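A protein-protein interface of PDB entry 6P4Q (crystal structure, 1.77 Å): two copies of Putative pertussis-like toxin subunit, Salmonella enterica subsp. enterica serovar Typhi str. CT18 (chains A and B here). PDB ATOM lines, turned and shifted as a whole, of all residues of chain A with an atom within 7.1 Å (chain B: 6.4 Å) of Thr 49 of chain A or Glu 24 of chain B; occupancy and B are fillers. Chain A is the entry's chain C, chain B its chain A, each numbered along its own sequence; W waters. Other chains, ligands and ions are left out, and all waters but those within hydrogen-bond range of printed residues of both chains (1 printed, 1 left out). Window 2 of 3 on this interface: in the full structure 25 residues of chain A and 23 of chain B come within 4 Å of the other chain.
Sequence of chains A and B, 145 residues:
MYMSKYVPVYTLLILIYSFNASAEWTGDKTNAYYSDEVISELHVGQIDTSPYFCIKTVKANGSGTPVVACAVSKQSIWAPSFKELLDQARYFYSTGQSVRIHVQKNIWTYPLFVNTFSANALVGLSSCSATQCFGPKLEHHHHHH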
ATOM      1  N   GLN A  46       7.491 -22.268   0.062  1.00  0.00           N
ATOM      2  CA  GLN A  46       8.553 -21.694  -0.763  1.00  0.00           C
ATOM      3  C   GLN A  46       9.622 -21.096   0.141  1.00  0.00           C
ATOM      4  O   GLN A  46       9.309 -20.573   1.211  1.00  0.00           O
ATOM      5  CB  GLN A  46       8.004 -20.610  -1.701  1.00  0.00           C
ATOM      6  CG  GLN A  46       9.013 -20.129  -2.732  1.00  0.00           C
ATOM      7  CD  GLN A  46       8.427 -19.150  -3.736  1.00  0.00           C
ATOM      8  OE1 GLN A  46       7.531 -19.487  -4.515  1.00  0.00           O
ATOM      9  NE2 GLN A  46       8.934 -17.926  -3.717  1.00  0.00           N
ATOM     10  N   ILE A  47      10.886 -21.188  -0.278  1.00  0.00           N
ATOM     11  CA  ILE A  47      11.978 -20.510   0.421  1.00  0.00           C
ATOM     12  C   ILE A  47      13.020 -20.065  -0.608  1.00  0.00           C
ATOM     13  O   ILE A  47      13.416 -20.843  -1.484  1.00  0.00           O
ATOM     14  CB  ILE A  47      12.586 -21.415   1.527  1.00  0.00           C
ATOM     15  CG1 ILE A  47      13.719 -20.690   2.274  1.00  0.00           C
ATOM     16  CG2 ILE A  47      13.059 -22.779   0.957  1.00  0.00           C
ATOM     17  CD1 ILE A  47      14.064 -21.318   3.636  1.00  0.00           C
ATOM     18  N   ASP A  48      13.453 -18.802  -0.510  1.00  0.00           N
ATOM     19  CA  ASP A  48      14.517 -18.268  -1.370  1.00  0.00           C
ATOM     20  C   ASP A  48      14.228 -18.537  -2.852  1.00  0.00           C
ATOM     21  O   ASP A  48      15.099 -18.980  -3.610  1.00  0.00           O
ATOM     22  CB  ASP A  48      15.876 -18.838  -0.966  1.00  0.00           C
ATOM     23  CG  ASP A  48      16.360 -18.286   0.342  1.00  0.00           C
ATOM     24  OD1 ASP A  48      16.132 -17.074   0.595  1.00  0.00           O
ATOM     25  OD2 ASP A  48      16.970 -19.053   1.116  1.00  0.00           O
ATOM     26  N   THR A  49      12.983 -18.252  -3.249  1.00  0.00           N
ATOM     27  CA  THR A  49      12.405 -18.377  -4.596  1.00  0.00           C
ATOM     28  C   THR A  49      12.176 -19.820  -5.023  1.00  0.00           C
ATOM     29  O   THR A  49      11.755 -20.061  -6.166  1.00  0.00           O
ATOM     30  CB  THR A  49      13.220 -17.654  -5.685  1.00  0.00           C
ATOM     31  OG1 THR A  49      14.413 -18.391  -5.995  1.00  0.00           O
ATOM     32  CG2 THR A  49      13.592 -16.246  -5.238  1.00  0.00           C
ATOM     33  N   SER A  50      12.397 -20.788  -4.140  1.00  0.00           N
ATOM     34  CA  SER A  50      12.274 -22.180  -4.525  1.00  0.00           C
ATOM     35  C   SER A  50      11.049 -22.805  -3.878  1.00  0.00           C
ATOM     36  O   SER A  50      10.976 -22.880  -2.640  1.00  0.00           O
ATOM     37  CB  SER A  50      13.530 -22.964  -4.134  1.00  0.00           C
ATOM     38  OG  SER A  50      13.356 -24.318  -4.514  1.00  0.00           O
ATOM     39  N   PRO A  51      10.093 -23.299  -4.658  1.00  0.00           N
ATOM     40  CA  PRO A  51       9.088 -24.194  -4.084  1.00  0.00           C
ATOM     41  C   PRO A  51       9.782 -25.332  -3.349  1.00  0.00           C
ATOM     42  O   PRO A  51      10.843 -25.805  -3.767  1.00  0.00           O
ATOM     43  CB  PRO A  51       8.317 -24.698  -5.311  1.00  0.00           C
ATOM     44  CG  PRO A  51       8.566 -23.660  -6.369  1.00  0.00           C
ATOM     45  CD  PRO A  51       9.969 -23.186  -6.121  1.00  0.00           C
ATOM     46  N   SER A  73      13.206 -27.203  -4.615  1.00  0.00           N
ATOM     47  CA  SER A  73      13.099 -27.412  -6.057  1.00  0.00           C
ATOM     48  C   SER A  73      14.384 -27.096  -6.815  1.00  0.00           C
ATOM     49  O   SER A  73      14.686 -27.750  -7.823  1.00  0.00           O
ATOM     50  CB  SER A  73      11.950 -26.583  -6.624  1.00  0.00           C
ATOM     51  OG  SER A  73      11.793 -26.929  -7.992  1.00  0.00           O
ATOM     52  N   LYS A  74      15.135 -26.084  -6.399  1.00  0.00           N
ATOM     53  CA  LYS A  74      16.343 -25.814  -7.177  1.00  0.00           C
ATOM     54  C   LYS A  74      17.572 -25.765  -6.287  1.00  0.00           C
ATOM     55  O   LYS A  74      18.511 -24.993  -6.540  1.00  0.00           O
ATOM     56  CB  LYS A  74      16.209 -24.526  -7.979  1.00  0.00           C
ATOM     57  CG  LYS A  74      15.729 -23.376  -7.149  1.00  0.00           C
ATOM     58  CD  LYS A  74      15.095 -22.298  -8.042  1.00  0.00           C
ATOM     59  CE  LYS A  74      15.271 -20.932  -7.426  1.00  0.00           C
ATOM     60  NZ  LYS A  74      15.348 -19.795  -8.429  1.00  0.00           N
ATOM     61  N   GLN A  75      17.581 -26.577  -5.237  1.00  0.00           N
ATOM     62  CA  GLN A  75      18.722 -26.651  -4.342  1.00  0.00           C
ATOM     63  C   GLN A  75      19.115 -28.107  -4.116  1.00  0.00           C
ATOM     64  O   GLN A  75      18.261 -29.005  -4.073  1.00  0.00           O
ATOM     65  CB  GLN A  75      18.429 -25.974  -3.004  1.00  0.00           C
ATOM     66  CG  GLN A  75      17.990 -24.531  -3.134  1.00  0.00           C
ATOM     67  CD  GLN A  75      17.951 -23.809  -1.800  1.00  0.00           C
ATOM     68  OE1 GLN A  75      18.712 -24.129  -0.879  1.00  0.00           O
ATOM     69  NE2 GLN A  75      17.067 -22.820  -1.691  1.00  0.00           N
ATOM     70  N   TYR A 110      19.045 -23.480   6.781  1.00  0.00           N
ATOM     71  CA  TYR A 110      18.410 -22.313   7.408  1.00  0.00           C
ATOM     72  C   TYR A 110      17.849 -22.723   8.764  1.00  0.00           C
ATOM     73  O   TYR A 110      16.948 -23.568   8.815  1.00  0.00           O
ATOM     74  CB  TYR A 110      17.297 -21.748   6.536  1.00  0.00           C
ATOM     75  CG  TYR A 110      16.711 -20.460   7.089  1.00  0.00           C
ATOM     76  CD1 TYR A 110      15.345 -20.333   7.305  1.00  0.00           C
ATOM     77  CD2 TYR A 110      17.532 -19.369   7.390  1.00  0.00           C
ATOM     78  CE1 TYR A 110      14.797 -19.156   7.807  1.00  0.00           C
ATOM     79  CE2 TYR A 110      16.991 -18.182   7.894  1.00  0.00           C
ATOM     80  CZ  TYR A 110      15.627 -18.083   8.093  1.00  0.00           C
ATOM     81  OH  TYR A 110      15.075 -16.920   8.583  1.00  0.00           O
ATOM     82  N   GLU B  24      12.920 -14.848   1.431  1.00  0.00           N
ATOM     83  CA  GLU B  24      11.539 -15.075   1.864  1.00  0.00           C
ATOM     84  C   GLU B  24      11.329 -16.546   2.201  1.00  0.00           C
ATOM     85  O   GLU B  24      12.061 -17.410   1.725  1.00  0.00           O
ATOM     86  CB  GLU B  24      10.565 -14.622   0.771  1.00  0.00           C
ATOM     87  CG  GLU B  24      10.145 -15.727  -0.194  1.00  0.00           C
ATOM     88  CD  GLU B  24      11.255 -16.248  -1.113  1.00  0.00           C
ATOM     89  OE1 GLU B  24      12.408 -15.770  -1.061  1.00  0.00           O
ATOM     90  OE2 GLU B  24      10.953 -17.179  -1.892  1.00  0.00           O
ATOM     91  N   TRP B  25      10.346 -16.821   3.053  1.00  0.00           N
ATOM     92  CA  TRP B  25      10.015 -18.193   3.405  1.00  0.00           C
ATOM     93  C   TRP B  25       8.579 -18.203   3.891  1.00  0.00           C
ATOM     94  O   TRP B  25       8.166 -17.299   4.617  1.00  0.00           O
ATOM     95  CB  TRP B  25      10.950 -18.737   4.495  1.00  0.00           C
ATOM     96  CG  TRP B  25      10.565 -20.081   5.057  1.00  0.00           C
ATOM     97  CD1 TRP B  25      10.116 -21.177   4.364  1.00  0.00           C
ATOM     98  CD2 TRP B  25      10.627 -20.473   6.437  1.00  0.00           C
ATOM     99  NE1 TRP B  25       9.904 -22.229   5.238  1.00  0.00           N
ATOM    100  CE2 TRP B  25      10.197 -21.812   6.514  1.00  0.00           C
ATOM    101  CE3 TRP B  25      11.003 -19.807   7.621  1.00  0.00           C
ATOM    102  CZ2 TRP B  25      10.135 -22.510   7.723  1.00  0.00           C
ATOM    103  CZ3 TRP B  25      10.933 -20.500   8.826  1.00  0.00           C
ATOM    104  CH2 TRP B  25      10.504 -21.843   8.863  1.00  0.00           C
ATOM    105  N   THR B  26       7.821 -19.212   3.461  1.00  0.00           N
ATOM    106  CA  THR B  26       6.504 -19.459   4.036  1.00  0.00           C
ATOM    107  C   THR B  26       6.456 -19.199   5.536  1.00  0.00           C
ATOM    108  O   THR B  26       5.522 -18.564   6.045  1.00  0.00           O
ATOM    109  CB  THR B  26       6.127 -20.906   3.758  1.00  0.00           C
ATOM    110  OG1 THR B  26       6.103 -21.107   2.344  1.00  0.00           O
ATOM    111  CG2 THR B  26       4.777 -21.237   4.387  1.00  0.00           C
ATOM    112  N   ASP B  28       8.401 -17.315   7.513  1.00  0.00           N
ATOM    113  CA  ASP B  28       8.811 -16.027   8.076  1.00  0.00           C
ATOM    114  C   ASP B  28       7.764 -15.532   9.059  1.00  0.00           C
ATOM    115  O   ASP B  28       6.569 -15.555   8.766  1.00  0.00           O
ATOM    116  CB  ASP B  28       8.977 -14.955   6.989  1.00  0.00           C
ATOM    117  CG  ASP B  28      10.159 -15.197   6.066  1.00  0.00           C
ATOM    118  OD1 ASP B  28      11.116 -15.911   6.446  1.00  0.00           O
ATOM    119  OD2 ASP B  28      10.122 -14.638   4.946  1.00  0.00           O
ATOM    120  N   ASN B  31       4.833 -13.326   8.064  1.00  0.00           N
ATOM    121  CA  ASN B  31       3.631 -13.865   7.449  1.00  0.00           C
ATOM    122  C   ASN B  31       2.610 -14.182   8.538  1.00  0.00           C
ATOM    123  O   ASN B  31       2.849 -13.975   9.729  1.00  0.00           O
ATOM    124  CB  ASN B  31       3.978 -15.080   6.596  1.00  0.00           C
ATOM    125  CG  ASN B  31       4.792 -14.697   5.394  1.00  0.00           C
ATOM    126  OD1 ASN B  31       4.550 -13.646   4.803  1.00  0.00           O
ATOM    127  ND2 ASN B  31       5.775 -15.533   5.026  1.00  0.00           N
ATOM    128  N   ILE B  77       6.823 -12.516  -5.523  1.00  0.00           N
ATOM    129  CA  ILE B  77       7.931 -13.434  -5.282  1.00  0.00           C
ATOM    130  C   ILE B  77       7.442 -14.871  -5.137  1.00  0.00           C
ATOM    131  O   ILE B  77       8.210 -15.810  -5.371  1.00  0.00           O
ATOM    132  CB  ILE B  77       8.743 -12.977  -4.046  1.00  0.00           C
ATOM    133  CG1 ILE B  77      10.058 -13.747  -3.961  1.00  0.00           C
ATOM    134  CG2 ILE B  77       7.931 -13.124  -2.750  1.00  0.00           C
ATOM    135  CD1 ILE B  77      11.124 -13.025  -3.133  1.00  0.00           C
ATOM    136  N   TRP B  78       6.162 -15.067  -4.796  1.00  0.00           N
ATOM    137  CA  TRP B  78       5.596 -16.398  -4.603  1.00  0.00           C
ATOM    138  C   TRP B  78       5.172 -17.073  -5.903  1.00  0.00           C
ATOM    139  O   TRP B  78       4.746 -18.229  -5.871  1.00  0.00           O
ATOM    140  CB  TRP B  78       4.388 -16.311  -3.668  1.00  0.00           C
ATOM    141  CG  TRP B  78       4.708 -15.587  -2.415  1.00  0.00           C
ATOM    142  CD1 TRP B  78       4.341 -14.313  -2.082  1.00  0.00           C
ATOM    143  CD2 TRP B  78       5.480 -16.089  -1.317  1.00  0.00           C
ATOM    144  NE1 TRP B  78       4.827 -13.998  -0.833  1.00  0.00           N
ATOM    145  CE2 TRP B  78       5.538 -15.068  -0.347  1.00  0.00           C
ATOM    146  CE3 TRP B  78       6.119 -17.314  -1.057  1.00  0.00           C
ATOM    147  CZ2 TRP B  78       6.207 -15.229   0.868  1.00  0.00           C
ATOM    148  CZ3 TRP B  78       6.783 -17.480   0.150  1.00  0.00           C
ATOM    149  CH2 TRP B  78       6.825 -16.436   1.100  1.00  0.00           C
ATOM    150  N   PRO B  80       6.668 -18.707  -8.293  1.00  0.00           N
ATOM    151  CA  PRO B  80       7.159 -20.056  -8.618  1.00  0.00           C
ATOM    152  C   PRO B  80       6.352 -21.188  -7.988  1.00  0.00           C
ATOM    153  O   PRO B  80       6.317 -22.280  -8.560  1.00  0.00           O
ATOM    154  CB  PRO B  80       8.603 -20.031  -8.091  1.00  0.00           C
ATOM    155  CG  PRO B  80       9.009 -18.605  -8.192  1.00  0.00           C
ATOM    156  CD  PRO B  80       7.761 -17.842  -7.799  1.00  0.00           C
ATOM    157  N   SER B  81       5.703 -20.963  -6.843  1.00  0.00           N
ATOM    158  CA  SER B  81       4.984 -22.016  -6.126  1.00  0.00           C
ATOM    159  C   SER B  81       3.515 -22.120  -6.530  1.00  0.00           C
ATOM    160  O   SER B  81       2.779 -22.919  -5.927  1.00  0.00           O
ATOM    161  CB  SER B  81       5.090 -21.784  -4.617  1.00  0.00           C
ATOM    162  OG  SER B  81       6.453 -21.835  -4.230  1.00  0.00           O
HETATM  163  O   HOH W   1      12.328 -16.679   8.733  1.00  0.00           O
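The side-chain amide nitrogen of Gln 46 of chain A lies within hydrogen-bond range of the side-chain carboxylate of Glu 24 of chain B, 2.8 Å away. N of Asp 48 of chain A is in hydrogen-bond range of O of Glu 24 of chain B (3.0 Å). The side-chain carboxylate of Glu 24 of chain B sits at hydrogen-bond distance from the backbone NH of Thr 49 of chain A (2.7 Å). N of Gln 46 of chain A is in hydrogen-bond range of OG1 of Thr 26 of chain B, 2.9 Å away. The side-chain amide nitrogen (NE2) of Gln 46 of chain A is in hydrogen-bond range of the backbone carbonyl oxygen (O) of Ile 77 of chain B (2.8 Å). The backbone carbonyl oxygen (O) of Trp 78 of chain B sits close to the side-chain amide oxygen (OE1) of Gln 46 of chain A (3.3 Å). OG of Ser 81 of chain B lies within hydrogen-bond range of OE1 of Gln 46 of chain A, 2.6 Å away.
The side-chain carboxylate (OD2) of Asp 28 of chain B is in hydrogen-bond range of the backbone NH (N) of Trp 25 of chain B, at 2.9 Å. The backbone carbonyl oxygen of Trp 25 of chain B sits at hydrogen-bond distance from the side-chain amide nitrogen of Asn 31 of chain B (3.0 Å). O of Thr 26 of chain B sits at hydrogen-bond distance from ND2 of Asn 31 of chain B (3.2 Å). OG1 of Thr 49 of chain A sits at hydrogen-bond distance from NZ of Lys 74 of chain A. O of Pro 51 of chain A sits at hydrogen-bond distance from N of Ser 73 of chain A, at 2.9 Å.
Among the printed residues, merely in contact across the chains: Gln 46 of chain A with Trp 25 of chain B, Gln 46 of chain A with Pro 80 of chain B, Ile 47 of chain A with Glu 24 of chain B, Ile 47 of chain A with Trp 25 of chain B, Thr 49 of chain A with Pro 80 of chain B, Pro 51 of chain A with Pro 80 of chain B, Pro 51 of chain A with Ser 81 of chain B and Tyr 110 of chain A with Trp 25 of chain B.
Thr 49 of chain A touches just these residues of chain B: Glu 24 and Pro 80. Of the printed residues of chain A, Glu 24 of chain B touches Gln 46, Ile 47, Asp 48 and Thr 49. Printed residues of chain A within 4 Å of Ile 77 of chain B: Gln 46. Of the printed residues of chain A, Pro 80 of chain B touches Gln 46, Thr 49 and Pro 51. Of the printed residues of chain B, Ile 47 of chain A touches Glu 24 and Trp 25. Asp 28 of chain B touches none of the printed residues of chain A. The nearest printed residue of chain B that does not touch Pro 51 of chain A is Trp 78 of chain B (6.7 Å).
Hydrophobic or aromatic side chains of chain B within 4 Å of the printed part of chain A: Trp 25, Trp 78 and Pro 80. Printed residues of chain A that touch a printed residue of chain B: Gln 46, Ile 47, Asp 48, Thr 49, Pro 51 and Tyr 110. Hydrophobic or aromatic side chains of chain A within 4 Å of the printed part of chain B: Ile 47, Pro 51 and Tyr 110. Among the printed residues, no Asp or Glu carboxylate lies within 4 Å of a Lys or Arg side-chain nitrogen of the other chain.
No position is printed for both chains.
Water W1 bridges OD1 of Asp 28 of chain B (2.7 Å) and OH of Tyr 110 of chain A (2.8 Å).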
